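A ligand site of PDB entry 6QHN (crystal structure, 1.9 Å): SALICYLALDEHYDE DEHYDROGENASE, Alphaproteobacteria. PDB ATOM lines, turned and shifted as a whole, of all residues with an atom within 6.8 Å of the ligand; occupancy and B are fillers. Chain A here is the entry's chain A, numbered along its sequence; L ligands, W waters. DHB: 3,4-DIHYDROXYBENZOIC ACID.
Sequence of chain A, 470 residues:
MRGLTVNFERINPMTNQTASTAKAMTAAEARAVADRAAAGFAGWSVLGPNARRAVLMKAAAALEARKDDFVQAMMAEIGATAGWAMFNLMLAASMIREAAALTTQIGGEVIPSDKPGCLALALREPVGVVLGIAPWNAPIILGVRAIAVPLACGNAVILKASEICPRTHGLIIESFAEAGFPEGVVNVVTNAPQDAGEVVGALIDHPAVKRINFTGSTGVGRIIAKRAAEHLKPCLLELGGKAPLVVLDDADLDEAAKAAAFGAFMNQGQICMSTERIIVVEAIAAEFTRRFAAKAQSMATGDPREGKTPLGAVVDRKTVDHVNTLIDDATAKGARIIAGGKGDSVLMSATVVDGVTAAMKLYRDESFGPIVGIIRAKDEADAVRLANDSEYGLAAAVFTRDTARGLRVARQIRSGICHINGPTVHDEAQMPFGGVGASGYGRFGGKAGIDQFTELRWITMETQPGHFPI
The side-chain amide nitrogen of Asn 137 sits at hydrogen-bond distance from an oxygen (O1) of the ligand (2.8 Å). An oxygen (O1) of the ligand lies within hydrogen-bond range of the backbone NH (N) of Cys 272, 3.4 Å away. The side-chain sulfur of Cys 272 lies within hydrogen-bond range of an oxygen (O2) of the ligand (2.8 Å).
The backbone carbonyl oxygen of Trp 84 sits at hydrogen-bond distance from the side-chain amide nitrogen of Asn 88 (3.2 Å). The backbone NH (N) of Ile 141 is in hydrogen-bond range of the side-chain amide oxygen (OD1) of Asn 88 (3.2 Å). N of His 426 lies within hydrogen-bond range of SD of Met 273. The backbone carbonyl oxygen of Gln 270 lies close to the side-chain amide nitrogen of Asn 137, at 3.2 Å. The backbone carbonyl oxygen (O) of Asn 137 is in hydrogen-bond range of the indole nitrogen (NE1) of Trp 84 (3.1 Å).
Trp 84 touches the ligand. Leu 91 touches the ligand. Ala 138 touches the ligand (CB to C2, 3.8 Å). Ile 141 touches the ligand. CD2 of Leu 142 touches O2 of the ligand, at 3.7 Å. Ile 271 touches the ligand. Met 273 touches the ligand (CE to C4, 3.5 Å). OD2 of Asp 427 touches C5 of the ligand, at 3.0 Å. Hydrophobic or aromatic side chains that line the ligand: Trp 84, Leu 91, Ala 138, Ile 141, Leu 142, Ile 271 and Met 273. Ten residues have an atom within 4 Å of the ligand: Trp 84, Leu 91, Asn 137, Ala 138, Ile 141, Leu 142, Ile 271, Cys 272, Met 273 and Asp 427.
Water W1 lies within hydrogen-bond range of O1 of the ligand, OD1 of Asn 137 and N of Cys 272. Water W2 lies within hydrogen-bond range of the guanidinium group (NH2) of Arg 145 (2.9 Å), the side-chain carboxylate (OE1) of Glu 238 (3.0 Å) and an oxygen (O2) of the ligand (3.1 Å).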
ATOM      1  N   TRP A  84     -11.624  38.153   7.768  1.00  0.00           N
ATOM      2  CA  TRP A  84     -11.497  36.699   7.525  1.00  0.00           C
ATOM      3  C   TRP A  84     -12.900  36.089   7.440  1.00  0.00           C
ATOM      4  O   TRP A  84     -13.133  35.252   6.556  1.00  0.00           O
ATOM      5  CB  TRP A  84     -10.642  36.021   8.621  1.00  0.00           C
ATOM      6  CG  TRP A  84     -10.452  34.533   8.444  1.00  0.00           C
ATOM      7  CD1 TRP A  84     -10.935  33.544   9.243  1.00  0.00           C
ATOM      8  CD2 TRP A  84      -9.785  33.879   7.370  1.00  0.00           C
ATOM      9  NE1 TRP A  84     -10.539  32.312   8.772  1.00  0.00           N
ATOM     10  CE2 TRP A  84      -9.833  32.491   7.614  1.00  0.00           C
ATOM     11  CE3 TRP A  84      -9.132  34.319   6.216  1.00  0.00           C
ATOM     12  CZ2 TRP A  84      -9.271  31.550   6.756  1.00  0.00           C
ATOM     13  CZ3 TRP A  84      -8.552  33.384   5.374  1.00  0.00           C
ATOM     14  CH2 TRP A  84      -8.627  32.023   5.652  1.00  0.00           C
ATOM     15  N   PHE A  87     -14.419  37.239   4.052  1.00  0.00           N
ATOM     16  CA  PHE A  87     -13.740  36.479   3.005  1.00  0.00           C
ATOM     17  C   PHE A  87     -14.317  35.049   2.921  1.00  0.00           C
ATOM     18  O   PHE A  87     -14.587  34.539   1.830  1.00  0.00           O
ATOM     19  CB  PHE A  87     -12.235  36.408   3.262  1.00  0.00           C
ATOM     20  CG  PHE A  87     -11.507  35.421   2.394  1.00  0.00           C
ATOM     21  CD1 PHE A  87     -11.342  35.651   1.033  1.00  0.00           C
ATOM     22  CD2 PHE A  87     -11.032  34.220   2.920  1.00  0.00           C
ATOM     23  CE1 PHE A  87     -10.729  34.688   0.206  1.00  0.00           C
ATOM     24  CE2 PHE A  87     -10.404  33.270   2.103  1.00  0.00           C
ATOM     25  CZ  PHE A  87     -10.275  33.504   0.750  1.00  0.00           C
ATOM     26  N   ASN A  88     -14.479  34.399   4.095  1.00  0.00           N
ATOM     27  CA  ASN A  88     -15.068  33.074   4.189  1.00  0.00           C
ATOM     28  C   ASN A  88     -16.477  33.078   3.560  1.00  0.00           C
ATOM     29  O   ASN A  88     -16.781  32.174   2.782  1.00  0.00           O
ATOM     30  CB  ASN A  88     -15.124  32.573   5.668  1.00  0.00           C
ATOM     31  CG  ASN A  88     -14.031  31.601   5.970  1.00  0.00           C
ATOM     32  OD1 ASN A  88     -14.230  30.404   5.909  1.00  0.00           O
ATOM     33  ND2 ASN A  88     -12.829  32.092   6.250  1.00  0.00           N
ATOM     34  N   LEU A  91     -16.276  33.689  -0.531  1.00  0.00           N
ATOM     35  CA  LEU A  91     -15.816  32.496  -1.240  1.00  0.00           C
ATOM     36  C   LEU A  91     -16.761  31.279  -1.072  1.00  0.00           C
ATOM     37  O   LEU A  91     -16.931  30.511  -2.020  1.00  0.00           O
ATOM     38  CB  LEU A  91     -14.406  32.105  -0.804  1.00  0.00           C
ATOM     39  CG  LEU A  91     -13.739  30.974  -1.627  1.00  0.00           C
ATOM     40  CD1 LEU A  91     -13.627  31.352  -3.114  1.00  0.00           C
ATOM     41  CD2 LEU A  91     -12.373  30.650  -1.089  1.00  0.00           C
ATOM     42  N   MET A  95     -18.585  29.185  -4.058  1.00  0.00           N
ATOM     43  CA  MET A  95     -18.501  27.728  -4.208  1.00  0.00           C
ATOM     44  C   MET A  95     -19.885  27.067  -4.341  1.00  0.00           C
ATOM     45  O   MET A  95     -20.021  26.075  -5.080  1.00  0.00           O
ATOM     46  CB  MET A  95     -17.767  27.101  -3.028  1.00  0.00           C
ATOM     47  CG  MET A  95     -16.310  27.522  -2.951  1.00  0.00           C
ATOM     48  SD  MET A  95     -15.691  27.330  -1.261  1.00  0.00           S
ATOM     49  CE  MET A  95     -15.697  25.597  -1.172  1.00  0.00           C
ATOM     50  N   PRO A 135     -13.669  21.145   9.395  1.00  0.00           N
ATOM     51  CA  PRO A 135     -12.926  21.725  10.513  1.00  0.00           C
ATOM     52  C   PRO A 135     -13.258  23.212  10.675  1.00  0.00           C
ATOM     53  O   PRO A 135     -14.083  23.756   9.939  1.00  0.00           O
ATOM     54  CB  PRO A 135     -11.467  21.442  10.102  1.00  0.00           C
ATOM     55  CG  PRO A 135     -11.461  21.581   8.660  1.00  0.00           C
ATOM     56  CD  PRO A 135     -12.881  21.286   8.156  1.00  0.00           C
ATOM     57  N   ASN A 137     -10.938  26.084  10.834  1.00  0.00           N
ATOM     58  CA  ASN A 137     -10.000  27.158  10.443  1.00  0.00           C
ATOM     59  C   ASN A 137     -10.520  28.136   9.377  1.00  0.00           C
ATOM     60  O   ASN A 137     -10.343  29.352   9.552  1.00  0.00           O
ATOM     61  CB  ASN A 137      -8.693  26.599  10.045  1.00  0.00           C
ATOM     62  CG  ASN A 137      -8.767  25.772   8.794  1.00  0.00           C
ATOM     63  OD1 ASN A 137      -9.316  24.670   8.803  1.00  0.00           O
ATOM     64  ND2 ASN A 137      -8.265  26.311   7.698  1.00  0.00           N
ATOM     65  N   ALA A 138     -11.255  27.632   8.364  1.00  0.00           N
ATOM     66  CA  ALA A 138     -11.904  28.431   7.313  1.00  0.00           C
ATOM     67  C   ALA A 138     -13.297  27.809   7.371  1.00  0.00           C
ATOM     68  O   ALA A 138     -13.568  26.840   6.665  1.00  0.00           O
ATOM     69  CB  ALA A 138     -11.207  28.190   5.975  1.00  0.00           C
ATOM     70  N   ILE A 141     -16.048  28.238   4.381  1.00  0.00           N
ATOM     71  CA  ILE A 141     -15.500  27.612   3.176  1.00  0.00           C
ATOM     72  C   ILE A 141     -15.566  26.084   3.263  1.00  0.00           C
ATOM     73  O   ILE A 141     -16.058  25.413   2.336  1.00  0.00           O
ATOM     74  CB  ILE A 141     -14.035  28.075   2.921  1.00  0.00           C
ATOM     75  CG1 ILE A 141     -14.027  29.543   2.427  1.00  0.00           C
ATOM     76  CG2 ILE A 141     -13.341  27.157   1.895  1.00  0.00           C
ATOM     77  CD1 ILE A 141     -12.684  30.285   2.608  1.00  0.00           C
ATOM     78  N   LEU A 142     -15.015  25.542   4.352  1.00  0.00           N
ATOM     79  CA  LEU A 142     -14.897  24.103   4.505  1.00  0.00           C
ATOM     80  C   LEU A 142     -16.174  23.414   4.882  1.00  0.00           C
ATOM     81  O   LEU A 142     -16.352  22.261   4.469  1.00  0.00           O
ATOM     82  CB  LEU A 142     -13.775  23.768   5.475  1.00  0.00           C
ATOM     83  CG  LEU A 142     -12.398  24.309   5.012  1.00  0.00           C
ATOM     84  CD1 LEU A 142     -11.343  24.094   6.083  1.00  0.00           C
ATOM     85  CD2 LEU A 142     -11.949  23.657   3.713  1.00  0.00           C
ATOM     86  N   ARG A 145     -17.812  23.356   1.540  1.00  0.00           N
ATOM     87  CA  ARG A 145     -17.108  22.401   0.657  1.00  0.00           C
ATOM     88  C   ARG A 145     -17.531  20.945   0.969  1.00  0.00           C
ATOM     89  O   ARG A 145     -17.676  20.118   0.051  1.00  0.00           O
ATOM     90  CB  ARG A 145     -15.580  22.521   0.830  1.00  0.00           C
ATOM     91  CG  ARG A 145     -14.802  21.712  -0.213  1.00  0.00           C
ATOM     92  CD  ARG A 145     -13.307  21.866  -0.083  1.00  0.00           C
ATOM     93  NE  ARG A 145     -12.749  21.211   1.096  1.00  0.00           N
ATOM     94  CZ  ARG A 145     -11.454  21.073   1.336  1.00  0.00           C
ATOM     95  NH1 ARG A 145     -10.557  21.555   0.477  1.00  0.00           N
ATOM     96  NH2 ARG A 145     -11.037  20.437   2.417  1.00  0.00           N
ATOM     97  N   THR A 215     -11.882  16.506   6.431  1.00  0.00           N
ATOM     98  CA  THR A 215     -10.773  17.453   6.390  1.00  0.00           C
ATOM     99  C   THR A 215     -10.341  17.608   7.855  1.00  0.00           C
ATOM    100  O   THR A 215     -11.164  17.910   8.705  1.00  0.00           O
ATOM    101  CB  THR A 215     -11.189  18.777   5.735  1.00  0.00           C
ATOM    102  OG1 THR A 215     -11.734  18.517   4.418  1.00  0.00           O
ATOM    103  CG2 THR A 215     -10.009  19.778   5.642  1.00  0.00           C
ATOM    104  N   GLU A 238      -8.563  14.835   3.272  1.00  0.00           N
ATOM    105  CA  GLU A 238      -7.744  16.048   3.073  1.00  0.00           C
ATOM    106  C   GLU A 238      -7.061  16.240   4.418  1.00  0.00           C
ATOM    107  O   GLU A 238      -7.727  16.717   5.326  1.00  0.00           O
ATOM    108  CB  GLU A 238      -8.671  17.237   2.868  1.00  0.00           C
ATOM    109  CG  GLU A 238      -9.423  17.236   1.560  1.00  0.00           C
ATOM    110  CD  GLU A 238      -8.535  17.552   0.393  1.00  0.00           C
ATOM    111  OE1 GLU A 238      -7.644  18.421   0.542  1.00  0.00           O
ATOM    112  OE2 GLU A 238      -8.733  16.929  -0.680  1.00  0.00           O
ATOM    113  N   GLN A 270      -3.133  29.375  10.275  1.00  0.00           N
ATOM    114  CA  GLN A 270      -4.044  28.278  10.617  1.00  0.00           C
ATOM    115  C   GLN A 270      -4.791  27.855   9.303  1.00  0.00           C
ATOM    116  O   GLN A 270      -5.992  28.079   9.157  1.00  0.00           O
ATOM    117  CB  GLN A 270      -5.046  28.746  11.693  1.00  0.00           C
ATOM    118  CG  GLN A 270      -4.352  29.325  12.949  1.00  0.00           C
ATOM    119  CD  GLN A 270      -5.327  29.843  13.972  1.00  0.00           C
ATOM    120  OE1 GLN A 270      -5.370  29.358  15.100  1.00  0.00           O
ATOM    121  NE2 GLN A 270      -6.135  30.835  13.620  1.00  0.00           N
ATOM    122  N   ILE A 271      -4.046  27.372   8.308  1.00  0.00           N
ATOM    123  CA  ILE A 271      -4.597  26.904   7.007  1.00  0.00           C
ATOM    124  C   ILE A 271      -3.820  25.619   6.693  1.00  0.00           C
ATOM    125  O   ILE A 271      -2.626  25.546   6.970  1.00  0.00           O
ATOM    126  CB  ILE A 271      -4.452  27.976   5.845  1.00  0.00           C
ATOM    127  CG1 ILE A 271      -4.925  29.376   6.327  1.00  0.00           C
ATOM    128  CG2 ILE A 271      -5.239  27.573   4.602  1.00  0.00           C
ATOM    129  CD1 ILE A 271      -4.905  30.496   5.285  1.00  0.00           C
ATOM    130  N   CYS A 272      -4.473  24.605   6.112  1.00  0.00           N
ATOM    131  CA  CYS A 272      -3.834  23.332   5.705  1.00  0.00           C
ATOM    132  C   CYS A 272      -2.650  23.570   4.762  1.00  0.00           C
ATOM    133  O   CYS A 272      -1.708  22.769   4.747  1.00  0.00           O
ATOM    134  CB  CYS A 272      -4.877  22.479   4.999  1.00  0.00           C
ATOM    135  SG  CYS A 272      -5.583  23.291   3.536  1.00  0.00           S
ATOM    136  N   MET A 273      -2.688  24.636   3.969  1.00  0.00           N
ATOM    137  CA  MET A 273      -1.711  24.988   2.934  1.00  0.00           C
ATOM    138  C   MET A 273      -0.864  26.231   3.318  1.00  0.00           C
ATOM    139  O   MET A 273      -0.201  26.795   2.447  1.00  0.00           O
ATOM    140  CB  MET A 273      -2.429  25.192   1.574  1.00  0.00           C
ATOM    141  CG  MET A 273      -3.603  26.153   1.632  1.00  0.00           C
ATOM    142  SD  MET A 273      -4.507  26.350   0.087  1.00  0.00           S
ATOM    143  CE  MET A 273      -6.023  26.994   0.721  1.00  0.00           C
ATOM    144  N   PHE A 368       0.465  24.997  12.718  1.00  0.00           N
ATOM    145  CA  PHE A 368      -0.865  25.631  12.646  1.00  0.00           C
ATOM    146  C   PHE A 368      -0.941  26.968  13.465  1.00  0.00           C
ATOM    147  O   PHE A 368      -1.884  27.199  14.202  1.00  0.00           O
ATOM    148  CB  PHE A 368      -1.963  24.619  13.028  1.00  0.00           C
ATOM    149  CG  PHE A 368      -3.104  24.588  12.036  1.00  0.00           C
ATOM    150  CD1 PHE A 368      -2.920  24.078  10.754  1.00  0.00           C
ATOM    151  CD2 PHE A 368      -4.366  25.038  12.380  1.00  0.00           C
ATOM    152  CE1 PHE A 368      -3.980  24.019   9.844  1.00  0.00           C
ATOM    153  CE2 PHE A 368      -5.414  25.003  11.461  1.00  0.00           C
ATOM    154  CZ  PHE A 368      -5.221  24.494  10.193  1.00  0.00           C
ATOM    155  N   LEU A 394       0.701  18.166   0.576  1.00  0.00           N
ATOM    156  CA  LEU A 394      -0.533  18.828   0.141  1.00  0.00           C
ATOM    157  C   LEU A 394      -0.178  19.911  -0.877  1.00  0.00           C
ATOM    158  O   LEU A 394      -0.193  19.620  -2.066  1.00  0.00           O
ATOM    159  CB  LEU A 394      -1.343  19.327   1.343  1.00  0.00           C
ATOM    160  CG  LEU A 394      -2.680  20.043   1.008  1.00  0.00           C
ATOM    161  CD1 LEU A 394      -3.562  19.179   0.104  1.00  0.00           C
ATOM    162  CD2 LEU A 394      -3.438  20.359   2.283  1.00  0.00           C
ATOM    163  N   VAL A 425      -0.855  29.267  -0.452  1.00  0.00           N
ATOM    164  CA  VAL A 425      -2.256  29.461  -0.091  1.00  0.00           C
ATOM    165  C   VAL A 425      -3.017  29.921  -1.333  1.00  0.00           C
ATOM    166  O   VAL A 425      -2.838  31.034  -1.808  1.00  0.00           O
ATOM    167  CB  VAL A 425      -2.416  30.459   1.075  1.00  0.00           C
ATOM    168  CG1 VAL A 425      -3.892  30.738   1.361  1.00  0.00           C
ATOM    169  CG2 VAL A 425      -1.708  29.935   2.345  1.00  0.00           C
ATOM    170  N   HIS A 426      -3.859  29.046  -1.869  1.00  0.00           N
ATOM    171  CA  HIS A 426      -4.605  29.327  -3.102  1.00  0.00           C
ATOM    172  C   HIS A 426      -5.611  28.204  -3.262  1.00  0.00           C
ATOM    173  O   HIS A 426      -5.250  27.041  -3.136  1.00  0.00           O
ATOM    174  CB  HIS A 426      -3.615  29.334  -4.313  1.00  0.00           C
ATOM    175  CG  HIS A 426      -4.197  29.581  -5.684  1.00  0.00           C
ATOM    176  ND1 HIS A 426      -3.404  29.470  -6.830  1.00  0.00           N
ATOM    177  CD2 HIS A 426      -5.439  29.976  -6.059  1.00  0.00           C
ATOM    178  CE1 HIS A 426      -4.213  29.735  -7.850  1.00  0.00           C
ATOM    179  NE2 HIS A 426      -5.439  30.038  -7.425  1.00  0.00           N
ATOM    180  N   ASP A 427      -6.868  28.557  -3.523  1.00  0.00           N
ATOM    181  CA  ASP A 427      -7.879  27.556  -3.836  1.00  0.00           C
ATOM    182  C   ASP A 427      -8.952  28.234  -4.665  1.00  0.00           C
ATOM    183  O   ASP A 427      -9.185  29.437  -4.526  1.00  0.00           O
ATOM    184  CB  ASP A 427      -8.482  26.951  -2.560  1.00  0.00           C
ATOM    185  CG  ASP A 427      -9.424  25.761  -2.815  1.00  0.00           C
ATOM    186  OD1 ASP A 427      -9.419  25.216  -3.941  1.00  0.00           O
ATOM    187  OD2 ASP A 427     -10.150  25.393  -1.884  1.00  0.00           O
ATOM    188  N   GLU A 428      -9.508  27.486  -5.597  1.00  0.00           N
ATOM    189  CA  GLU A 428     -10.615  27.932  -6.467  1.00  0.00           C
ATOM    190  C   GLU A 428     -11.504  26.720  -6.618  1.00  0.00           C
ATOM    191  O   GLU A 428     -11.011  25.602  -6.756  1.00  0.00           O
ATOM    192  CB  GLU A 428     -10.099  28.435  -7.825  1.00  0.00           C
ATOM    193  CG  GLU A 428      -9.129  29.603  -7.728  1.00  0.00           C
ATOM    194  CD  GLU A 428      -8.703  30.156  -9.076  1.00  0.00           C
ATOM    195  OE1 GLU A 428      -9.570  30.608  -9.848  1.00  0.00           O
ATOM    196  OE2 GLU A 428      -7.480  30.118  -9.372  1.00  0.00           O
ATOM    197  N   PHE A 433      -8.359  19.719  -5.668  1.00  0.00           N
ATOM    198  CA  PHE A 433      -7.599  20.046  -4.464  1.00  0.00           C
ATOM    199  C   PHE A 433      -7.498  18.836  -3.545  1.00  0.00           C
ATOM    200  O   PHE A 433      -8.502  18.363  -3.041  1.00  0.00           O
ATOM    201  CB  PHE A 433      -8.316  21.216  -3.742  1.00  0.00           C
ATOM    202  CG  PHE A 433      -7.525  21.857  -2.615  1.00  0.00           C
ATOM    203  CD1 PHE A 433      -7.425  21.222  -1.377  1.00  0.00           C
ATOM    204  CD2 PHE A 433      -6.980  23.123  -2.753  1.00  0.00           C
ATOM    205  CE1 PHE A 433      -6.687  21.806  -0.323  1.00  0.00           C
ATOM    206  CE2 PHE A 433      -6.270  23.715  -1.690  1.00  0.00           C
ATOM    207  CZ  PHE A 433      -6.130  23.053  -0.494  1.00  0.00           C
HETATM  208  C1  DHB L   1      -8.592  25.586   3.118  1.00  0.00           C
HETATM  209  C2  DHB L   1      -8.609  26.944   3.456  1.00  0.00           C
HETATM  210  C3  DHB L   1      -8.982  27.901   2.539  1.00  0.00           C
HETATM  211  O3  DHB L   1      -8.942  29.220   2.918  1.00  0.00           O
HETATM  212  C4  DHB L   1      -9.407  27.508   1.279  1.00  0.00           C
HETATM  213  O4  DHB L   1      -9.774  28.471   0.385  1.00  0.00           O
HETATM  214  C5  DHB L   1      -9.420  26.147   0.933  1.00  0.00           C
HETATM  215  C6  DHB L   1      -9.008  25.177   1.847  1.00  0.00           C
HETATM  216  C   DHB L   1      -8.172  24.613   4.169  1.00  0.00           C
HETATM  217  O1  DHB L   1      -7.709  25.067   5.241  1.00  0.00           O
HETATM  218  O2  DHB L   1      -8.303  23.381   3.948  1.00  0.00           O
HETATM  219  O   HOH W   1      -7.470  23.095   7.100  1.00  0.00           O
HETATM  220  O   HOH W   2      -8.194  20.605   2.591  1.00  0.00           O
